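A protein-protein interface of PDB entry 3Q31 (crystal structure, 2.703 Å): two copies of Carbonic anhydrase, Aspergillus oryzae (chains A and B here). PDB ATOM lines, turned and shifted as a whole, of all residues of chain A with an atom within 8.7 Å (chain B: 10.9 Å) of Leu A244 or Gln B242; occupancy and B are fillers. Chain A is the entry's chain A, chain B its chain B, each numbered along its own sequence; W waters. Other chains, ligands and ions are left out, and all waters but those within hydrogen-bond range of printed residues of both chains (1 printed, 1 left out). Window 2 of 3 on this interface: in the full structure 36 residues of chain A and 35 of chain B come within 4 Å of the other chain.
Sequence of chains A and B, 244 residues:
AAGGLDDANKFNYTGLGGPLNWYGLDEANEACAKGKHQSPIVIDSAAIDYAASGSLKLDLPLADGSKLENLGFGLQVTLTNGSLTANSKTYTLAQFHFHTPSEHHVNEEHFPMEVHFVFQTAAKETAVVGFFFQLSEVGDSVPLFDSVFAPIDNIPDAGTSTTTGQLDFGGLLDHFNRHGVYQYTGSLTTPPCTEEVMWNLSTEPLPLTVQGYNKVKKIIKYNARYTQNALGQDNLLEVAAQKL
The backbone carbonyl oxygen of Tyr A23 is in hydrogen-bond range of the side-chain amino group of Lys B243 (3.4 Å).
The side-chain hydroxyl (OH) of Tyr A23 is in hydrogen-bond range of the side-chain amino group (NZ) of Lys A34, at 3.3 Å. The side-chain amide oxygen (OD1) of Asn B235 lies within hydrogen-bond range of the backbone NH (N) of Leu B237 (2.9 Å). O of Glu B238 sits close to OE1 of Gln B242, 2.4 Å away.
Leu B236 touches Leu A20 (CD1 to CB, 3.6 Å). CB of Ala B240 touches O of Leu A20 (3.4 Å). Val B239 touches Asn A21 (CG1 to OD1, 3.8 Å). Lys B243 touches Gly A24 (NZ to CA, 3.9997 Å). CB of Ala B240 touches CD2 of Leu A237, 3.5 Å away. Ala A240 touches Leu B237. CG of Glu B238 touches OXT of Leu A244, at 3.5 Å. Ala B241 touches Leu A244 (CB to O, 3.7 Å). NE2 of Gln B242 touches O of Leu A244 (3.6 Å).
Printed residues of chain B within 4 Å of Ala A240: Leu B237. No residue of chain B comes within 4 Å of Lys A243. Of chain B, only Glu B238 (3.5 Å), Ala B241 (3.7 Å) and Gln B242 (3.6 Å) come within 4 Å of Leu A244. Of the printed residues of chain A, Leu B236 touches Leu A20 (3.6 Å). Printed residues of chain A within 4 Å of Leu B237: Ala A240 (3.5 Å). Printed residues of chain A within 4 Å of Ala B240: Leu A20 and Leu A237. Ala B241 touches just one residue of chain A: Leu A244 (3.7 Å). Of chain A, only Leu A244 (3.6 Å) comes within 4 Å of Gln B242. Leu B244 touches none of the printed residues of chain A. The nearest residue of chain A that does not touch Gln B242 is Tyr A23 (5.7 Å).
Of the 12 printed residues of chain A, 7 touch a printed residue of chain B. Among the printed residues, 10 pairs touch across the chains. Among the printed residues, no Asp or Glu carboxylate lies within 4 Å of a Lys or Arg side-chain nitrogen of the other chain.
Tyr A23 touches Lys B243, but with the chains exchanged Lys A243 does not touch Tyr B23 (5.0 Å). Leu A237 touches Ala B240, and with the chains exchanged Ala A240 touches Leu B237. Leu A244 touches Ala B241, but with the chains exchanged Ala A241 does not touch Leu B244 (5.8 Å). Leu A244 touches Gln B242, but with the chains exchanged Gln A242 does not touch Leu B244 (8.3 Å). Of the 10 pairs that touch across the chains among the printed residues, 2 have their exchanged pair printed and touching as well.
Water W1 lies within hydrogen-bond range of O of Leu B244, NZ of Lys A243 and O of Ala A241.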
ATOM      1  N   LEU A  20     -29.860  21.585  21.310  1.00  0.00           N
ATOM      2  CA  LEU A  20     -29.029  22.690  20.870  1.00  0.00           C
ATOM      3  C   LEU A  20     -27.589  22.252  20.733  1.00  0.00           C
ATOM      4  O   LEU A  20     -26.806  22.885  20.027  1.00  0.00           O
ATOM      5  CB  LEU A  20     -29.147  23.892  21.802  1.00  0.00           C
ATOM      6  CG  LEU A  20     -30.485  24.589  21.574  1.00  0.00           C
ATOM      7  CD1 LEU A  20     -31.437  24.214  22.692  1.00  0.00           C
ATOM      8  CD2 LEU A  20     -30.316  26.091  21.470  1.00  0.00           C
ATOM      9  N   ASN A  21     -27.244  21.157  21.394  1.00  0.00           N
ATOM     10  CA  ASN A  21     -25.880  20.652  21.324  1.00  0.00           C
ATOM     11  C   ASN A  21     -25.793  19.174  20.959  1.00  0.00           C
ATOM     12  O   ASN A  21     -24.957  18.458  21.491  1.00  0.00           O
ATOM     13  CB  ASN A  21     -25.156  20.907  22.650  1.00  0.00           C
ATOM     14  CG  ASN A  21     -23.692  20.491  22.615  1.00  0.00           C
ATOM     15  OD1 ASN A  21     -22.949  20.823  21.680  1.00  0.00           O
ATOM     16  ND2 ASN A  21     -23.268  19.768  23.646  1.00  0.00           N
ATOM     17  N   TYR A  23     -25.175  18.079  17.855  1.00  0.00           N
ATOM     18  CA  TYR A  23     -24.088  17.991  16.891  1.00  0.00           C
ATOM     19  C   TYR A  23     -22.769  17.878  17.613  1.00  0.00           C
ATOM     20  O   TYR A  23     -21.863  17.170  17.167  1.00  0.00           O
ATOM     21  CB  TYR A  23     -24.061  19.240  16.030  1.00  0.00           C
ATOM     22  CG  TYR A  23     -23.003  19.245  14.948  1.00  0.00           C
ATOM     23  CD1 TYR A  23     -22.740  18.104  14.196  1.00  0.00           C
ATOM     24  CD2 TYR A  23     -22.298  20.407  14.648  1.00  0.00           C
ATOM     25  CE1 TYR A  23     -21.793  18.121  13.195  1.00  0.00           C
ATOM     26  CE2 TYR A  23     -21.356  20.428  13.647  1.00  0.00           C
ATOM     27  CZ  TYR A  23     -21.103  19.287  12.924  1.00  0.00           C
ATOM     28  OH  TYR A  23     -20.160  19.323  11.925  1.00  0.00           O
ATOM     29  N   GLY A  24     -22.665  18.595  18.726  1.00  0.00           N
ATOM     30  CA  GLY A  24     -21.452  18.618  19.513  1.00  0.00           C
ATOM     31  C   GLY A  24     -21.303  17.330  20.279  1.00  0.00           C
ATOM     32  O   GLY A  24     -20.255  17.081  20.870  1.00  0.00           O
ATOM     33  N   ALA A  33     -28.035  20.134  13.243  1.00  0.00           N
ATOM     34  CA  ALA A  33     -27.602  21.519  13.315  1.00  0.00           C
ATOM     35  C   ALA A  33     -27.535  22.224  11.957  1.00  0.00           C
ATOM     36  O   ALA A  33     -27.703  23.441  11.891  1.00  0.00           O
ATOM     37  CB  ALA A  33     -26.263  21.604  14.039  1.00  0.00           C
ATOM     38  N   LYS A  34     -27.295  21.483  10.874  1.00  0.00           N
ATOM     39  CA  LYS A  34     -27.131  22.126   9.569  1.00  0.00           C
ATOM     40  C   LYS A  34     -28.279  21.837   8.607  1.00  0.00           C
ATOM     41  O   LYS A  34     -28.327  22.398   7.514  1.00  0.00           O
ATOM     42  CB  LYS A  34     -25.780  21.780   8.920  1.00  0.00           C
ATOM     43  CG  LYS A  34     -24.559  21.899   9.854  1.00  0.00           C
ATOM     44  CD  LYS A  34     -23.203  21.712   9.140  1.00  0.00           C
ATOM     45  CE  LYS A  34     -22.042  21.555  10.152  1.00  0.00           C
ATOM     46  NZ  LYS A  34     -20.654  21.522   9.568  1.00  0.00           N
ATOM     47  N   LEU A 237     -30.055  27.174  13.976  1.00  0.00           N
ATOM     48  CA  LEU A 237     -28.876  27.245  14.833  1.00  0.00           C
ATOM     49  C   LEU A 237     -27.761  27.888  14.031  1.00  0.00           C
ATOM     50  O   LEU A 237     -26.981  28.697  14.546  1.00  0.00           O
ATOM     51  CB  LEU A 237     -28.406  25.864  15.266  1.00  0.00           C
ATOM     52  CG  LEU A 237     -29.084  25.196  16.453  1.00  0.00           C
ATOM     53  CD1 LEU A 237     -29.640  23.817  16.044  1.00  0.00           C
ATOM     54  CD2 LEU A 237     -28.085  25.102  17.608  1.00  0.00           C
ATOM     55  N   ALA A 240     -28.526  31.397  14.202  1.00  0.00           N
ATOM     56  CA  ALA A 240     -28.022  31.936  15.450  1.00  0.00           C
ATOM     57  C   ALA A 240     -26.509  32.057  15.459  1.00  0.00           C
ATOM     58  O   ALA A 240     -25.947  32.773  16.290  1.00  0.00           O
ATOM     59  CB  ALA A 240     -28.477  31.079  16.602  1.00  0.00           C
ATOM     60  N   ALA A 241     -25.852  31.371  14.533  1.00  0.00           N
ATOM     61  CA  ALA A 241     -24.394  31.279  14.566  1.00  0.00           C
ATOM     62  C   ALA A 241     -23.636  32.542  14.102  1.00  0.00           C
ATOM     63  O   ALA A 241     -22.419  32.518  13.943  1.00  0.00           O
ATOM     64  CB  ALA A 241     -23.913  30.027  13.841  1.00  0.00           C
ATOM     65  N   GLN A 242     -24.337  33.668  13.978  1.00  0.00           N
ATOM     66  CA  GLN A 242     -23.669  34.982  13.893  1.00  0.00           C
ATOM     67  C   GLN A 242     -24.035  35.924  15.061  1.00  0.00           C
ATOM     68  O   GLN A 242     -25.097  36.558  15.056  1.00  0.00           O
ATOM     69  CB  GLN A 242     -23.974  35.665  12.566  1.00  0.00           C
ATOM     70  CG  GLN A 242     -25.395  35.463  12.100  1.00  0.00           C
ATOM     71  CD  GLN A 242     -25.566  34.146  11.361  1.00  0.00           C
ATOM     72  OE1 GLN A 242     -24.809  33.184  11.576  1.00  0.00           O
ATOM     73  NE2 GLN A 242     -26.564  34.096  10.474  1.00  0.00           N
ATOM     74  N   LYS A 243     -23.120  36.061  16.020  1.00  0.00           N
ATOM     75  CA  LYS A 243     -21.751  35.550  15.874  1.00  0.00           C
ATOM     76  C   LYS A 243     -21.218  34.859  17.139  1.00  0.00           C
ATOM     77  O   LYS A 243     -21.990  34.491  18.040  1.00  0.00           O
ATOM     78  CB  LYS A 243     -20.779  36.694  15.478  1.00  0.00           C
ATOM     79  CG  LYS A 243     -20.567  36.928  13.966  1.00  0.00           C
ATOM     80  CD  LYS A 243     -20.255  35.618  13.236  1.00  0.00           C
ATOM     81  CE  LYS A 243     -19.088  34.871  13.895  1.00  0.00           C
ATOM     82  NZ  LYS A 243     -19.323  33.396  13.975  1.00  0.00           N
ATOM     83  N   LEU A 244     -19.888  34.691  17.155  1.00  0.00           N
ATOM     84  CA  LEU A 244     -19.062  34.292  18.314  1.00  0.00           C
ATOM     85  C   LEU A 244     -19.483  32.984  19.001  1.00  0.00           C
ATOM     86  O   LEU A 244     -18.864  31.924  18.812  1.00  0.00           O
ATOM     87  CB  LEU A 244     -18.947  35.443  19.344  1.00  0.00           C
ATOM     88  CG  LEU A 244     -17.611  35.759  20.050  1.00  0.00           C
ATOM     89  CD1 LEU A 244     -17.747  37.013  20.924  1.00  0.00           C
ATOM     90  CD2 LEU A 244     -17.047  34.571  20.867  1.00  0.00           C
ATOM     91  OXT LEU A 244     -20.447  32.966  19.774  1.00  0.00           O
ATOM     92  N   TYR B  23     -31.714  37.470  19.648  1.00  0.00           N
ATOM     93  CA  TYR B  23     -30.581  38.384  19.567  1.00  0.00           C
ATOM     94  C   TYR B  23     -30.534  39.035  18.200  1.00  0.00           C
ATOM     95  O   TYR B  23     -30.195  40.217  18.061  1.00  0.00           O
ATOM     96  CB  TYR B  23     -29.274  37.639  19.804  1.00  0.00           C
ATOM     97  CG  TYR B  23     -28.036  38.517  19.801  1.00  0.00           C
ATOM     98  CD1 TYR B  23     -28.030  39.761  20.428  1.00  0.00           C
ATOM     99  CD2 TYR B  23     -26.857  38.082  19.198  1.00  0.00           C
ATOM    100  CE1 TYR B  23     -26.885  40.552  20.442  1.00  0.00           C
ATOM    101  CE2 TYR B  23     -25.708  38.862  19.209  1.00  0.00           C
ATOM    102  CZ  TYR B  23     -25.728  40.093  19.835  1.00  0.00           C
ATOM    103  OH  TYR B  23     -24.587  40.863  19.848  1.00  0.00           O
ATOM    104  N   GLU B  27     -30.169  44.085  18.813  1.00  0.00           N
ATOM    105  CA  GLU B  27     -28.914  43.937  19.549  1.00  0.00           C
ATOM    106  C   GLU B  27     -29.097  44.076  21.060  1.00  0.00           C
ATOM    107  O   GLU B  27     -28.221  43.686  21.841  1.00  0.00           O
ATOM    108  CB  GLU B  27     -27.876  44.942  19.045  1.00  0.00           C
ATOM    109  CG  GLU B  27     -26.572  44.968  19.863  1.00  0.00           C
ATOM    110  CD  GLU B  27     -25.575  43.864  19.478  1.00  0.00           C
ATOM    111  OE1 GLU B  27     -25.732  43.235  18.403  1.00  0.00           O
ATOM    112  OE2 GLU B  27     -24.615  43.643  20.255  1.00  0.00           O
ATOM    113  N   GLU B  30     -28.574  40.786  23.652  1.00  0.00           N
ATOM    114  CA  GLU B  30     -27.335  40.052  23.898  1.00  0.00           C
ATOM    115  C   GLU B  30     -27.458  38.957  24.943  1.00  0.00           C
ATOM    116  O   GLU B  30     -26.965  37.844  24.751  1.00  0.00           O
ATOM    117  CB  GLU B  30     -26.207  40.994  24.308  1.00  0.00           C
ATOM    118  CG  GLU B  30     -25.348  41.404  23.143  1.00  0.00           C
ATOM    119  CD  GLU B  30     -24.059  42.052  23.577  1.00  0.00           C
ATOM    120  OE1 GLU B  30     -23.052  41.313  23.691  1.00  0.00           O
ATOM    121  OE2 GLU B  30     -24.057  43.289  23.794  1.00  0.00           O
ATOM    122  N   CYS B  32     -29.885  37.163  25.879  1.00  0.00           N
ATOM    123  CA  CYS B  32     -30.641  36.025  25.387  1.00  0.00           C
ATOM    124  C   CYS B  32     -29.692  34.982  24.852  1.00  0.00           C
ATOM    125  O   CYS B  32     -29.869  33.792  25.062  1.00  0.00           O
ATOM    126  CB  CYS B  32     -31.577  36.454  24.266  1.00  0.00           C
ATOM    127  SG  CYS B  32     -32.998  37.440  24.771  1.00  0.00           S
ATOM    128  N   ALA B  33     -28.666  35.450  24.159  1.00  0.00           N
ATOM    129  CA  ALA B  33     -27.759  34.563  23.456  1.00  0.00           C
ATOM    130  C   ALA B  33     -26.378  34.417  24.121  1.00  0.00           C
ATOM    131  O   ALA B  33     -25.721  33.385  23.960  1.00  0.00           O
ATOM    132  CB  ALA B  33     -27.620  35.008  21.995  1.00  0.00           C
ATOM    133  N   LYS B  34     -25.932  35.426  24.866  1.00  0.00           N
ATOM    134  CA  LYS B  34     -24.595  35.356  25.454  1.00  0.00           C
ATOM    135  C   LYS B  34     -24.616  35.141  26.965  1.00  0.00           C
ATOM    136  O   LYS B  34     -23.575  34.912  27.564  1.00  0.00           O
ATOM    137  CB  LYS B  34     -23.748  36.596  25.083  1.00  0.00           C
ATOM    138  CG  LYS B  34     -23.762  36.962  23.591  1.00  0.00           C
ATOM    139  CD  LYS B  34     -22.729  38.038  23.186  1.00  0.00           C
ATOM    140  CE  LYS B  34     -23.002  38.533  21.738  1.00  0.00           C
ATOM    141  NZ  LYS B  34     -22.000  39.477  21.140  1.00  0.00           N
ATOM    142  N   GLY B  35     -25.792  35.203  27.581  1.00  0.00           N
ATOM    143  CA  GLY B  35     -25.891  35.102  29.029  1.00  0.00           C
ATOM    144  C   GLY B  35     -25.505  33.753  29.608  1.00  0.00           C
ATOM    145  O   GLY B  35     -25.892  32.715  29.075  1.00  0.00           O
ATOM    146  N   LYS B  36     -24.755  33.761  30.704  1.00  0.00           N
ATOM    147  CA  LYS B  36     -24.424  32.527  31.414  1.00  0.00           C
ATOM    148  C   LYS B  36     -25.373  32.219  32.570  1.00  0.00           C
ATOM    149  O   LYS B  36     -25.161  31.240  33.296  1.00  0.00           O
ATOM    150  CB  LYS B  36     -23.005  32.579  31.974  1.00  0.00           C
ATOM    151  CG  LYS B  36     -21.930  32.153  31.014  1.00  0.00           C
ATOM    152  CD  LYS B  36     -21.560  33.247  30.032  1.00  0.00           C
ATOM    153  CE  LYS B  36     -20.182  32.962  29.436  1.00  0.00           C
ATOM    154  NZ  LYS B  36     -19.214  32.510  30.499  1.00  0.00           N
ATOM    155  N   ASN B 229     -28.537  26.281  29.599  1.00  0.00           N
ATOM    156  CA  ASN B 229     -27.396  25.592  30.137  1.00  0.00           C
ATOM    157  C   ASN B 229     -27.442  25.784  31.640  1.00  0.00           C
ATOM    158  O   ASN B 229     -28.314  26.466  32.151  1.00  0.00           O
ATOM    159  CB  ASN B 229     -26.104  26.143  29.543  1.00  0.00           C
ATOM    160  CG  ASN B 229     -24.957  25.116  29.551  1.00  0.00           C
ATOM    161  OD1 ASN B 229     -24.988  24.102  30.267  1.00  0.00           O
ATOM    162  ND2 ASN B 229     -23.931  25.393  28.756  1.00  0.00           N
ATOM    163  N   GLN B 233     -22.578  28.379  33.213  1.00  0.00           N
ATOM    164  CA  GLN B 233     -22.134  27.770  31.966  1.00  0.00           C
ATOM    165  C   GLN B 233     -22.504  28.606  30.767  1.00  0.00           C
ATOM    166  O   GLN B 233     -23.509  29.320  30.795  1.00  0.00           O
ATOM    167  CB  GLN B 233     -22.743  26.384  31.809  1.00  0.00           C
ATOM    168  CG  GLN B 233     -22.282  25.434  32.876  1.00  0.00           C
ATOM    169  CD  GLN B 233     -20.789  25.518  33.075  1.00  0.00           C
ATOM    170  OE1 GLN B 233     -20.306  25.586  34.208  1.00  0.00           O
ATOM    171  NE2 GLN B 233     -20.045  25.530  31.967  1.00  0.00           N
ATOM    172  N   ASP B 234     -21.704  28.500  29.711  1.00  0.00           N
ATOM    173  CA  ASP B 234     -21.925  29.275  28.492  1.00  0.00           C
ATOM    174  C   ASP B 234     -23.337  29.141  27.971  1.00  0.00           C
ATOM    175  O   ASP B 234     -23.901  28.055  27.933  1.00  0.00           O
ATOM    176  CB  ASP B 234     -20.979  28.836  27.382  1.00  0.00           C
ATOM    177  CG  ASP B 234     -19.541  28.798  27.826  1.00  0.00           C
ATOM    178  OD1 ASP B 234     -19.136  27.766  28.412  1.00  0.00           O
ATOM    179  OD2 ASP B 234     -18.823  29.795  27.583  1.00  0.00           O
ATOM    180  N   ASN B 235     -23.911  30.259  27.556  1.00  0.00           N
ATOM    181  CA  ASN B 235     -25.208  30.205  26.925  1.00  0.00           C
ATOM    182  C   ASN B 235     -25.085  29.100  25.910  1.00  0.00           C
ATOM    183  O   ASN B 235     -24.117  29.060  25.151  1.00  0.00           O
ATOM    184  CB  ASN B 235     -25.532  31.520  26.229  1.00  0.00           C
ATOM    185  CG  ASN B 235     -26.955  31.572  25.718  1.00  0.00           C
ATOM    186  OD1 ASN B 235     -27.356  30.781  24.860  1.00  0.00           O
ATOM    187  ND2 ASN B 235     -27.726  32.517  26.235  1.00  0.00           N
ATOM    188  N   LEU B 236     -26.036  28.180  25.903  1.00  0.00           N
ATOM    189  CA  LEU B 236     -25.860  27.057  25.026  1.00  0.00           C
ATOM    190  C   LEU B 236     -26.288  27.367  23.594  1.00  0.00           C
ATOM    191  O   LEU B 236     -26.674  26.471  22.846  1.00  0.00           O
ATOM    192  CB  LEU B 236     -26.447  25.760  25.603  1.00  0.00           C
ATOM    193  CG  LEU B 236     -27.879  25.747  26.092  1.00  0.00           C
ATOM    194  CD1 LEU B 236     -28.806  25.787  24.896  1.00  0.00           C
ATOM    195  CD2 LEU B 236     -28.110  24.498  26.914  1.00  0.00           C
ATOM    196  N   LEU B 237     -26.187  28.639  23.212  1.00  0.00           N
ATOM    197  CA  LEU B 237     -26.213  29.014  21.797  1.00  0.00           C
ATOM    198  C   LEU B 237     -24.784  29.318  21.380  1.00  0.00           C
ATOM    199  O   LEU B 237     -24.352  28.987  20.279  1.00  0.00           O
ATOM    200  CB  LEU B 237     -27.076  30.253  21.567  1.00  0.00           C
ATOM    201  CG  LEU B 237     -28.579  30.057  21.419  1.00  0.00           C
ATOM    202  CD1 LEU B 237     -29.303  30.946  22.403  1.00  0.00           C
ATOM    203  CD2 LEU B 237     -29.018  30.344  20.000  1.00  0.00           C
ATOM    204  N   GLU B 238     -24.052  29.972  22.272  1.00  0.00           N
ATOM    205  CA  GLU B 238     -22.652  30.224  22.031  1.00  0.00           C
ATOM    206  C   GLU B 238     -21.924  28.901  21.976  1.00  0.00           C
ATOM    207  O   GLU B 238     -20.950  28.768  21.245  1.00  0.00           O
ATOM    208  CB  GLU B 238     -22.064  31.085  23.133  1.00  0.00           C
ATOM    209  CG  GLU B 238     -22.089  32.561  22.842  1.00  0.00           C
ATOM    210  CD  GLU B 238     -21.465  33.354  23.970  1.00  0.00           C
ATOM    211  OE1 GLU B 238     -20.960  34.463  23.690  1.00  0.00           O
ATOM    212  OE2 GLU B 238     -21.470  32.866  25.132  1.00  0.00           O
ATOM    213  N   VAL B 239     -22.405  27.929  22.751  1.00  0.00           N
ATOM    214  CA  VAL B 239     -21.869  26.573  22.704  1.00  0.00           C
ATOM    215  C   VAL B 239     -22.065  25.982  21.316  1.00  0.00           C
ATOM    216  O   VAL B 239     -21.131  25.473  20.699  1.00  0.00           O
ATOM    217  CB  VAL B 239     -22.548  25.677  23.732  1.00  0.00           C
ATOM    218  CG1 VAL B 239     -22.375  24.202  23.359  1.00  0.00           C
ATOM    219  CG2 VAL B 239     -21.995  25.964  25.121  1.00  0.00           C
ATOM    220  N   ALA B 240     -23.289  26.076  20.823  1.00  0.00           N
ATOM    221  CA  ALA B 240     -23.611  25.609  19.477  1.00  0.00           C
ATOM    222  C   ALA B 240     -22.872  26.370  18.377  1.00  0.00           C
ATOM    223  O   ALA B 240     -22.772  25.904  17.242  1.00  0.00           O
ATOM    224  CB  ALA B 240     -25.109  25.702  19.247  1.00  0.00           C
ATOM    225  N   ALA B 241     -22.361  27.546  18.715  1.00  0.00           N
ATOM    226  CA  ALA B 241     -21.782  28.429  17.717  1.00  0.00           C
ATOM    227  C   ALA B 241     -20.360  28.037  17.366  1.00  0.00           C
ATOM    228  O   ALA B 241     -19.822  28.508  16.363  1.00  0.00           O
ATOM    229  CB  ALA B 241     -21.813  29.843  18.209  1.00  0.00           C
ATOM    230  N   GLN B 242     -19.723  27.265  18.251  1.00  0.00           N
ATOM    231  CA  GLN B 242     -18.476  26.599  17.903  1.00  0.00           C
ATOM    232  C   GLN B 242     -18.967  25.491  17.014  1.00  0.00           C
ATOM    233  O   GLN B 242     -19.804  24.691  17.430  1.00  0.00           O
ATOM    234  CB  GLN B 242     -17.777  26.025  19.129  1.00  0.00           C
ATOM    235  CG  GLN B 242     -18.366  26.475  20.446  1.00  0.00           C
ATOM    236  CD  GLN B 242     -18.224  27.978  20.666  1.00  0.00           C
ATOM    237  OE1 GLN B 242     -18.598  28.506  21.724  1.00  0.00           O
ATOM    238  NE2 GLN B 242     -17.677  28.677  19.668  1.00  0.00           N
ATOM    239  N   LYS B 243     -18.458  25.462  15.791  1.00  0.00           N
ATOM    240  CA  LYS B 243     -19.089  24.744  14.688  1.00  0.00           C
ATOM    241  C   LYS B 243     -19.951  25.750  13.904  1.00  0.00           C
ATOM    242  O   LYS B 243     -21.178  25.762  13.981  1.00  0.00           O
ATOM    243  CB  LYS B 243     -19.872  23.502  15.161  1.00  0.00           C
ATOM    244  CG  LYS B 243     -19.030  22.524  16.020  1.00  0.00           C
ATOM    245  CD  LYS B 243     -19.553  21.066  16.034  1.00  0.00           C
ATOM    246  CE  LYS B 243     -18.458  20.053  16.464  1.00  0.00           C
ATOM    247  NZ  LYS B 243     -18.846  18.586  16.479  1.00  0.00           N
ATOM    248  N   LEU B 244     -19.251  26.621  13.186  1.00  0.00           N
ATOM    249  CA  LEU B 244     -17.782  26.563  13.251  1.00  0.00           C
ATOM    250  C   LEU B 244     -17.132  27.775  13.923  1.00  0.00           C
ATOM    251  O   LEU B 244     -17.508  28.918  13.646  1.00  0.00           O
ATOM    252  CB  LEU B 244     -17.147  26.272  11.885  1.00  0.00           C
ATOM    253  CG  LEU B 244     -15.882  25.414  12.032  1.00  0.00           C
ATOM    254  CD1 LEU B 244     -15.667  24.536  10.797  1.00  0.00           C
ATOM    255  CD2 LEU B 244     -14.640  26.266  12.378  1.00  0.00           C
ATOM    256  OXT LEU B 244     -16.223  27.619  14.756  1.00  0.00           O
HETATM  257  O   HOH W   1     -20.079  30.454  13.045  1.00  0.00           O
